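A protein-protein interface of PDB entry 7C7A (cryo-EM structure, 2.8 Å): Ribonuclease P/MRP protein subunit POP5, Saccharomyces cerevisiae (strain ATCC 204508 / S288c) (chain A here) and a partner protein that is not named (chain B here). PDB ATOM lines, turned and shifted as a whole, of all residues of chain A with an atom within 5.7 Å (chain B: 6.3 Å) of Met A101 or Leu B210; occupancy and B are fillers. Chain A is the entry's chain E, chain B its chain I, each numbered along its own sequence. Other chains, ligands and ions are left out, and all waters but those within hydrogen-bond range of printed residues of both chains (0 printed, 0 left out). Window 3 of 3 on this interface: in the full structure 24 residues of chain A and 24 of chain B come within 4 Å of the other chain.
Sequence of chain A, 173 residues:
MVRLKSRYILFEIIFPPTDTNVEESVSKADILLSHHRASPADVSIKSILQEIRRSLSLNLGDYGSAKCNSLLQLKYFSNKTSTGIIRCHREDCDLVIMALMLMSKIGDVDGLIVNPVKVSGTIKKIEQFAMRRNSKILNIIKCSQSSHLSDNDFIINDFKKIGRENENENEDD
Printed residues of chain B within 4 Å of Ile A97: Leu B205 (3.5 Å), Gly B206 (3.7 Å) and Ser B209 (3.3 Å).
Of chain B, only Arg B202 (2.4 Å), Gly B206 (3.2 Å), Val B207 (3.7 Å) and Leu B210 (3.7 Å) come within 4 Å of Met A101.
Of the printed residues of chain B, Leu A102 touches Leu B164 (3.7 Å).
Printed residues of chain B within 4 Å of Met A103: Arg B202 (3.1 Å).
Printed residues of chain A within 4 Å of Arg B202: Met A101 (2.4 Å) and Met A103 (3.1 Å).
Printed residues of chain A within 4 Å of Ser B209: Ile A97 (3.3 Å) and Met A98 (3.3 Å).
The nearest printed residue of chain B that does not touch Pro A116 is Gly B206 (4.1 Å).
Of the 17 printed residues of chain B, 9 touch a printed residue of chain A.
Along chain B the printed residues that touch a printed residue of chain A span positions 164 to 213.
Printed residues of chain A that touch a printed residue of chain B: Ile A97, Met A98, Met A101, Leu A102, Met A103 and Pro A116.
Among the printed residues, no Asp or Glu carboxylate lies within 4 Å of a Lys or Arg side-chain nitrogen of the other chain.
The backbone carbonyl oxygen (O) of Gly B206 lies within hydrogen-bond range of the side-chain hydroxyl (OG) of Ser B209 (2.7 Å).
The backbone carbonyl oxygen (O) of Leu B205 is in hydrogen-bond range of the side-chain hydroxyl (OG) of Ser B209, 3.4 Å away.
The side-chain amide nitrogen of Asn B213 is in hydrogen-bond range of the backbone carbonyl oxygen of Ser B209, 3.3 Å away.
SD of Met A101 lies close to O of Gly B206, 3.2 Å away.
The backbone carbonyl oxygen of Met A103 sits at hydrogen-bond distance from the guanidinium group of Arg B202 (3.1 Å).
ND2 of Asn B213 lies within hydrogen-bond range of SD of Met A98, at 3.2 Å.
The side-chain sulfur (SD) of Met A101 sits at hydrogen-bond distance from the backbone NH (N) of Val B207 (3.7 Å).
O of Met A101 sits at hydrogen-bond distance from NE of Arg B202, at 2.4 Å.
The backbone NH (N) of Met A98 sits at hydrogen-bond distance from the side-chain hydroxyl (OG) of Ser B209, at 3.3 Å.
The backbone carbonyl oxygen of Pro A116 lies within hydrogen-bond range of the side-chain amide nitrogen of Asn B203, 3.4 Å away.
Leu B205 touches Ile A97.
Ile A97 touches Gly B206.
Ile A97 touches Ser B209.
CA of Leu B210 touches SD of Met A98, at 3.7 Å.
CE of Met A101 touches CB of Leu B210, at 3.7 Å.
CD2 of Leu B164 touches CD2 of Leu A102, 3.7 Å away.
O of Pro A116 touches CD1 of Leu B205, 3.4 Å away.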
ATOM      1  N   VAL A  96      22.678  13.563 -17.200  1.00  0.00           N
ATOM      2  CA  VAL A  96      23.289  13.982 -18.457  1.00  0.00           C
ATOM      3  C   VAL A  96      22.832  13.080 -19.598  1.00  0.00           C
ATOM      4  O   VAL A  96      22.611  13.546 -20.722  1.00  0.00           O
ATOM      5  CB  VAL A  96      24.824  13.999 -18.325  1.00  0.00           C
ATOM      6  CG1 VAL A  96      25.465  14.456 -19.629  1.00  0.00           C
ATOM      7  CG2 VAL A  96      25.249  14.890 -17.167  1.00  0.00           C
ATOM      8  N   ILE A  97      22.671  11.782 -19.330  1.00  0.00           N
ATOM      9  CA  ILE A  97      22.207  10.870 -20.373  1.00  0.00           C
ATOM     10  C   ILE A  97      20.779  11.206 -20.787  1.00  0.00           C
ATOM     11  O   ILE A  97      20.457  11.241 -21.982  1.00  0.00           O
ATOM     12  CB  ILE A  97      22.333   9.409 -19.904  1.00  0.00           C
ATOM     13  CG1 ILE A  97      23.804   8.999 -19.820  1.00  0.00           C
ATOM     14  CG2 ILE A  97      21.582   8.477 -20.843  1.00  0.00           C
ATOM     15  CD1 ILE A  97      24.018   7.574 -19.363  1.00  0.00           C
ATOM     16  N   MET A  98      19.901  11.460 -19.813  1.00  0.00           N
ATOM     17  CA  MET A  98      18.526  11.823 -20.137  1.00  0.00           C
ATOM     18  C   MET A  98      18.457  13.159 -20.867  1.00  0.00           C
ATOM     19  O   MET A  98      17.611  13.338 -21.752  1.00  0.00           O
ATOM     20  CB  MET A  98      17.676  11.867 -18.867  1.00  0.00           C
ATOM     21  CG  MET A  98      16.178  11.812 -19.126  1.00  0.00           C
ATOM     22  SD  MET A  98      15.193  11.912 -17.620  1.00  0.00           S
ATOM     23  CE  MET A  98      15.526  13.597 -17.119  1.00  0.00           C
ATOM     24  N   ALA A  99      19.333  14.105 -20.519  1.00  0.00           N
ATOM     25  CA  ALA A  99      19.366  15.373 -21.241  1.00  0.00           C
ATOM     26  C   ALA A  99      19.845  15.189 -22.674  1.00  0.00           C
ATOM     27  O   ALA A  99      19.288  15.798 -23.595  1.00  0.00           O
ATOM     28  CB  ALA A  99      20.256  16.376 -20.509  1.00  0.00           C
ATOM     29  N   LEU A 100      20.871  14.361 -22.885  1.00  0.00           N
ATOM     30  CA  LEU A 100      21.331  14.084 -24.241  1.00  0.00           C
ATOM     31  C   LEU A 100      20.270  13.352 -25.050  1.00  0.00           C
ATOM     32  O   LEU A 100      20.193  13.526 -26.271  1.00  0.00           O
ATOM     33  CB  LEU A 100      22.624  13.271 -24.207  1.00  0.00           C
ATOM     34  CG  LEU A 100      23.904  14.049 -23.896  1.00  0.00           C
ATOM     35  CD1 LEU A 100      25.045  13.092 -23.592  1.00  0.00           C
ATOM     36  CD2 LEU A 100      24.265  14.971 -25.051  1.00  0.00           C
ATOM     37  N   MET A 101      19.451  12.529 -24.392  1.00  0.00           N
ATOM     38  CA  MET A 101      18.339  11.891 -25.088  1.00  0.00           C
ATOM     39  C   MET A 101      17.263  12.908 -25.452  1.00  0.00           C
ATOM     40  O   MET A 101      16.708  12.866 -26.555  1.00  0.00           O
ATOM     41  CB  MET A 101      17.748  10.774 -24.230  1.00  0.00           C
ATOM     42  CG  MET A 101      16.515  10.124 -24.836  1.00  0.00           C
ATOM     43  SD  MET A 101      15.337   9.535 -23.606  1.00  0.00           S
ATOM     44  CE  MET A 101      15.148  10.999 -22.594  1.00  0.00           C
ATOM     45  N   LEU A 102      16.959  13.827 -24.538  1.00  0.00           N
ATOM     46  CA  LEU A 102      15.929  14.837 -24.751  1.00  0.00           C
ATOM     47  C   LEU A 102      16.413  16.026 -25.575  1.00  0.00           C
ATOM     48  O   LEU A 102      15.719  17.048 -25.618  1.00  0.00           O
ATOM     49  CB  LEU A 102      15.393  15.326 -23.403  1.00  0.00           C
ATOM     50  CG  LEU A 102      14.239  14.520 -22.805  1.00  0.00           C
ATOM     51  CD1 LEU A 102      13.732  15.170 -21.528  1.00  0.00           C
ATOM     52  CD2 LEU A 102      13.112  14.364 -23.813  1.00  0.00           C
ATOM     53  N   MET A 103      17.574  15.926 -26.220  1.00  0.00           N
ATOM     54  CA  MET A 103      18.070  17.008 -27.067  1.00  0.00           C
ATOM     55  C   MET A 103      17.205  17.098 -28.317  1.00  0.00           C
ATOM     56  O   MET A 103      17.113  16.139 -29.089  1.00  0.00           O
ATOM     57  CB  MET A 103      19.534  16.773 -27.429  1.00  0.00           C
ATOM     58  CG  MET A 103      20.189  17.951 -28.135  1.00  0.00           C
ATOM     59  SD  MET A 103      21.985  17.959 -27.976  1.00  0.00           S
ATOM     60  CE  MET A 103      22.176  18.390 -26.248  1.00  0.00           C
ATOM     61  N   VAL A 114      20.833  12.492 -30.991  1.00  0.00           N
ATOM     62  CA  VAL A 114      22.019  12.270 -30.174  1.00  0.00           C
ATOM     63  C   VAL A 114      21.956  10.856 -29.615  1.00  0.00           C
ATOM     64  O   VAL A 114      20.946  10.462 -29.019  1.00  0.00           O
ATOM     65  CB  VAL A 114      22.130  13.304 -29.039  1.00  0.00           C
ATOM     66  CG1 VAL A 114      23.383  13.054 -28.213  1.00  0.00           C
ATOM     67  CG2 VAL A 114      22.131  14.714 -29.608  1.00  0.00           C
ATOM     68  N   PRO A 116      23.946   8.254 -27.101  1.00  0.00           N
ATOM     69  CA  PRO A 116      25.013   7.917 -26.145  1.00  0.00           C
ATOM     70  C   PRO A 116      25.474   6.482 -26.365  1.00  0.00           C
ATOM     71  O   PRO A 116      24.669   5.551 -26.343  1.00  0.00           O
ATOM     72  CB  PRO A 116      24.334   8.091 -24.781  1.00  0.00           C
ATOM     73  CG  PRO A 116      22.885   7.851 -25.053  1.00  0.00           C
ATOM     74  CD  PRO A 116      22.621   8.323 -26.459  1.00  0.00           C
ATOM     75  N   TYR B 160       7.221   6.136 -24.822  1.00  0.00           N
ATOM     76  CA  TYR B 160       8.148   7.242 -24.589  1.00  0.00           C
ATOM     77  C   TYR B 160       8.277   8.170 -25.792  1.00  0.00           C
ATOM     78  O   TYR B 160       8.993   9.177 -25.698  1.00  0.00           O
ATOM     79  CB  TYR B 160       9.525   6.705 -24.187  1.00  0.00           C
ATOM     80  CG  TYR B 160      10.340   6.115 -25.321  1.00  0.00           C
ATOM     81  CD1 TYR B 160      11.208   6.904 -26.068  1.00  0.00           C
ATOM     82  CD2 TYR B 160      10.253   4.765 -25.632  1.00  0.00           C
ATOM     83  CE1 TYR B 160      11.953   6.369 -27.100  1.00  0.00           C
ATOM     84  CE2 TYR B 160      10.999   4.220 -26.661  1.00  0.00           C
ATOM     85  CZ  TYR B 160      11.847   5.025 -27.391  1.00  0.00           C
ATOM     86  OH  TYR B 160      12.590   4.487 -28.416  1.00  0.00           O
ATOM     87  N   ALA B 163       6.168  11.887 -25.803  1.00  0.00           N
ATOM     88  CA  ALA B 163       6.739  13.042 -25.117  1.00  0.00           C
ATOM     89  C   ALA B 163       7.542  13.912 -26.077  1.00  0.00           C
ATOM     90  O   ALA B 163       7.695  15.120 -25.861  1.00  0.00           O
ATOM     91  CB  ALA B 163       7.612  12.577 -23.951  1.00  0.00           C
ATOM     92  N   LEU B 164       8.066  13.314 -27.146  1.00  0.00           N
ATOM     93  CA  LEU B 164       8.978  14.019 -28.039  1.00  0.00           C
ATOM     94  C   LEU B 164       8.241  14.827 -29.101  1.00  0.00           C
ATOM     95  O   LEU B 164       8.875  15.408 -29.990  1.00  0.00           O
ATOM     96  CB  LEU B 164       9.929  13.026 -28.711  1.00  0.00           C
ATOM     97  CG  LEU B 164      10.883  12.256 -27.795  1.00  0.00           C
ATOM     98  CD1 LEU B 164      11.646  11.202 -28.580  1.00  0.00           C
ATOM     99  CD2 LEU B 164      11.840  13.208 -27.098  1.00  0.00           C
ATOM    100  N   PHE B 173       2.005  13.558 -20.079  1.00  0.00           N
ATOM    101  CA  PHE B 173       2.683  12.276 -20.230  1.00  0.00           C
ATOM    102  C   PHE B 173       3.419  11.880 -18.957  1.00  0.00           C
ATOM    103  O   PHE B 173       3.361  10.718 -18.543  1.00  0.00           O
ATOM    104  CB  PHE B 173       3.658  12.326 -21.407  1.00  0.00           C
ATOM    105  CG  PHE B 173       4.711  11.255 -21.363  1.00  0.00           C
ATOM    106  CD1 PHE B 173       4.397   9.943 -21.679  1.00  0.00           C
ATOM    107  CD2 PHE B 173       6.012  11.559 -20.999  1.00  0.00           C
ATOM    108  CE1 PHE B 173       5.363   8.956 -21.636  1.00  0.00           C
ATOM    109  CE2 PHE B 173       6.983  10.575 -20.957  1.00  0.00           C
ATOM    110  CZ  PHE B 173       6.657   9.272 -21.275  1.00  0.00           C
ATOM    111  N   ARG B 202      15.414   7.203 -30.320  1.00  0.00           N
ATOM    112  CA  ARG B 202      16.470   7.248 -29.320  1.00  0.00           C
ATOM    113  C   ARG B 202      17.041   5.853 -29.093  1.00  0.00           C
ATOM    114  O   ARG B 202      16.572   4.860 -29.654  1.00  0.00           O
ATOM    115  CB  ARG B 202      15.952   7.839 -28.003  1.00  0.00           C
ATOM    116  CG  ARG B 202      15.482   9.279 -28.126  1.00  0.00           C
ATOM    117  CD  ARG B 202      16.621  10.183 -28.568  1.00  0.00           C
ATOM    118  NE  ARG B 202      16.245  11.593 -28.554  1.00  0.00           N
ATOM    119  CZ  ARG B 202      15.716  12.236 -29.589  1.00  0.00           C
ATOM    120  NH1 ARG B 202      15.407  13.522 -29.485  1.00  0.00           N
ATOM    121  NH2 ARG B 202      15.494  11.595 -30.728  1.00  0.00           N
ATOM    122  N   ASN B 203      18.072   5.791 -28.253  1.00  0.00           N
ATOM    123  CA  ASN B 203      18.816   4.570 -27.980  1.00  0.00           C
ATOM    124  C   ASN B 203      18.388   3.981 -26.639  1.00  0.00           C
ATOM    125  O   ASN B 203      17.480   4.481 -25.968  1.00  0.00           O
ATOM    126  CB  ASN B 203      20.321   4.847 -28.006  1.00  0.00           C
ATOM    127  CG  ASN B 203      21.135   3.622 -28.384  1.00  0.00           C
ATOM    128  OD1 ASN B 203      20.586   2.602 -28.801  1.00  0.00           O
ATOM    129  ND2 ASN B 203      22.451   3.719 -28.239  1.00  0.00           N
ATOM    130  N   LEU B 205      20.289   3.646 -23.829  1.00  0.00           N
ATOM    131  CA  LEU B 205      20.793   4.339 -22.645  1.00  0.00           C
ATOM    132  C   LEU B 205      19.888   5.498 -22.246  1.00  0.00           C
ATOM    133  O   LEU B 205      19.530   5.638 -21.069  1.00  0.00           O
ATOM    134  CB  LEU B 205      22.218   4.833 -22.893  1.00  0.00           C
ATOM    135  CG  LEU B 205      23.298   3.762 -23.054  1.00  0.00           C
ATOM    136  CD1 LEU B 205      24.673   4.400 -23.182  1.00  0.00           C
ATOM    137  CD2 LEU B 205      23.265   2.784 -21.889  1.00  0.00           C
ATOM    138  N   GLY B 206      19.512   6.339 -23.206  1.00  0.00           N
ATOM    139  CA  GLY B 206      18.654   7.473 -22.928  1.00  0.00           C
ATOM    140  C   GLY B 206      17.283   7.076 -22.423  1.00  0.00           C
ATOM    141  O   GLY B 206      16.782   7.655 -21.454  1.00  0.00           O
ATOM    142  N   VAL B 207      16.666   6.086 -23.072  1.00  0.00           N
ATOM    143  CA  VAL B 207      15.349   5.625 -22.644  1.00  0.00           C
ATOM    144  C   VAL B 207      15.427   5.002 -21.257  1.00  0.00           C
ATOM    145  O   VAL B 207      14.537   5.201 -20.420  1.00  0.00           O
ATOM    146  CB  VAL B 207      14.769   4.644 -23.679  1.00  0.00           C
ATOM    147  CG1 VAL B 207      13.471   4.032 -23.172  1.00  0.00           C
ATOM    148  CG2 VAL B 207      14.547   5.348 -25.006  1.00  0.00           C
ATOM    149  N   THR B 208      16.493   4.243 -20.989  1.00  0.00           N
ATOM    150  CA  THR B 208      16.667   3.651 -19.667  1.00  0.00           C
ATOM    151  C   THR B 208      16.808   4.728 -18.601  1.00  0.00           C
ATOM    152  O   THR B 208      16.183   4.643 -17.538  1.00  0.00           O
ATOM    153  CB  THR B 208      17.886   2.728 -19.661  1.00  0.00           C
ATOM    154  OG1 THR B 208      17.719   1.706 -20.654  1.00  0.00           O
ATOM    155  CG2 THR B 208      18.055   2.076 -18.296  1.00  0.00           C
ATOM    156  N   SER B 209      17.612   5.760 -18.873  1.00  0.00           N
ATOM    157  CA  SER B 209      17.770   6.845 -17.910  1.00  0.00           C
ATOM    158  C   SER B 209      16.460   7.595 -17.701  1.00  0.00           C
ATOM    159  O   SER B 209      16.132   7.981 -16.572  1.00  0.00           O
ATOM    160  CB  SER B 209      18.869   7.803 -18.373  1.00  0.00           C
ATOM    161  OG  SER B 209      18.491   8.472 -19.564  1.00  0.00           O
ATOM    162  N   LEU B 210      15.692   7.802 -18.774  1.00  0.00           N
ATOM    163  CA  LEU B 210      14.413   8.494 -18.655  1.00  0.00           C
ATOM    164  C   LEU B 210      13.440   7.705 -17.788  1.00  0.00           C
ATOM    165  O   LEU B 210      12.837   8.249 -16.855  1.00  0.00           O
ATOM    166  CB  LEU B 210      13.821   8.742 -20.042  1.00  0.00           C
ATOM    167  CG  LEU B 210      12.372   9.233 -20.087  1.00  0.00           C
ATOM    168  CD1 LEU B 210      12.272  10.666 -19.587  1.00  0.00           C
ATOM    169  CD2 LEU B 210      11.809   9.112 -21.494  1.00  0.00           C
ATOM    170  N   ILE B 211      13.273   6.412 -18.082  1.00  0.00           N
ATOM    171  CA  ILE B 211      12.361   5.590 -17.296  1.00  0.00           C
ATOM    172  C   ILE B 211      12.858   5.415 -15.865  1.00  0.00           C
ATOM    173  O   ILE B 211      12.047   5.253 -14.947  1.00  0.00           O
ATOM    174  CB  ILE B 211      12.143   4.228 -17.983  1.00  0.00           C
ATOM    175  CG1 ILE B 211      11.681   4.428 -19.427  1.00  0.00           C
ATOM    176  CG2 ILE B 211      11.097   3.413 -17.246  1.00  0.00           C
ATOM    177  CD1 ILE B 211      10.355   5.147 -19.550  1.00  0.00           C
ATOM    178  N   LYS B 212      14.174   5.470 -15.644  1.00  0.00           N
ATOM    179  CA  LYS B 212      14.697   5.379 -14.285  1.00  0.00           C
ATOM    180  C   LYS B 212      14.399   6.646 -13.496  1.00  0.00           C
ATOM    181  O   LYS B 212      14.000   6.578 -12.327  1.00  0.00           O
ATOM    182  CB  LYS B 212      16.200   5.110 -14.322  1.00  0.00           C
ATOM    183  CG  LYS B 212      16.768   4.570 -13.022  1.00  0.00           C
ATOM    184  CD  LYS B 212      18.282   4.479 -13.085  1.00  0.00           C
ATOM    185  CE  LYS B 212      18.746   3.813 -14.371  1.00  0.00           C
ATOM    186  NZ  LYS B 212      20.223   3.902 -14.543  1.00  0.00           N
ATOM    187  N   ASN B 213      14.587   7.813 -14.115  1.00  0.00           N
ATOM    188  CA  ASN B 213      14.244   9.070 -13.464  1.00  0.00           C
ATOM    189  C   ASN B 213      12.742   9.254 -13.308  1.00  0.00           C
ATOM    190  O   ASN B 213      12.312  10.042 -12.459  1.00  0.00           O
ATOM    191  CB  ASN B 213      14.830  10.247 -14.247  1.00  0.00           C
ATOM    192  CG  ASN B 213      16.342  10.314 -14.156  1.00  0.00           C
ATOM    193  OD1 ASN B 213      16.933   9.909 -13.156  1.00  0.00           O
ATOM    194  ND2 ASN B 213      16.976  10.827 -15.205  1.00  0.00           N
ATOM    195  N   LEU B 214      11.939   8.546 -14.104  1.00  0.00           N
ATOM    196  CA  LEU B 214      10.489   8.640 -13.985  1.00  0.00           C
ATOM    197  C   LEU B 214       9.937   7.825 -12.823  1.00  0.00           C
ATOM    198  O   LEU B 214       8.811   8.082 -12.386  1.00  0.00           O
ATOM    199  CB  LEU B 214       9.824   8.198 -15.290  1.00  0.00           C
ATOM    200  CG  LEU B 214       9.753   9.259 -16.391  1.00  0.00           C
ATOM    201  CD1 LEU B 214       9.191   8.669 -17.675  1.00  0.00           C
ATOM    202  CD2 LEU B 214       8.928  10.453 -15.937  1.00  0.00           C
ATOM    203  N   GLY B 215      10.694   6.853 -12.313  1.00  0.00           N
ATOM    204  CA  GLY B 215      10.247   6.089 -11.165  1.00  0.00           C
ATOM    205  C   GLY B 215      10.474   4.593 -11.257  1.00  0.00           C
ATOM    206  O   GLY B 215      10.042   3.845 -10.375  1.00  0.00           O
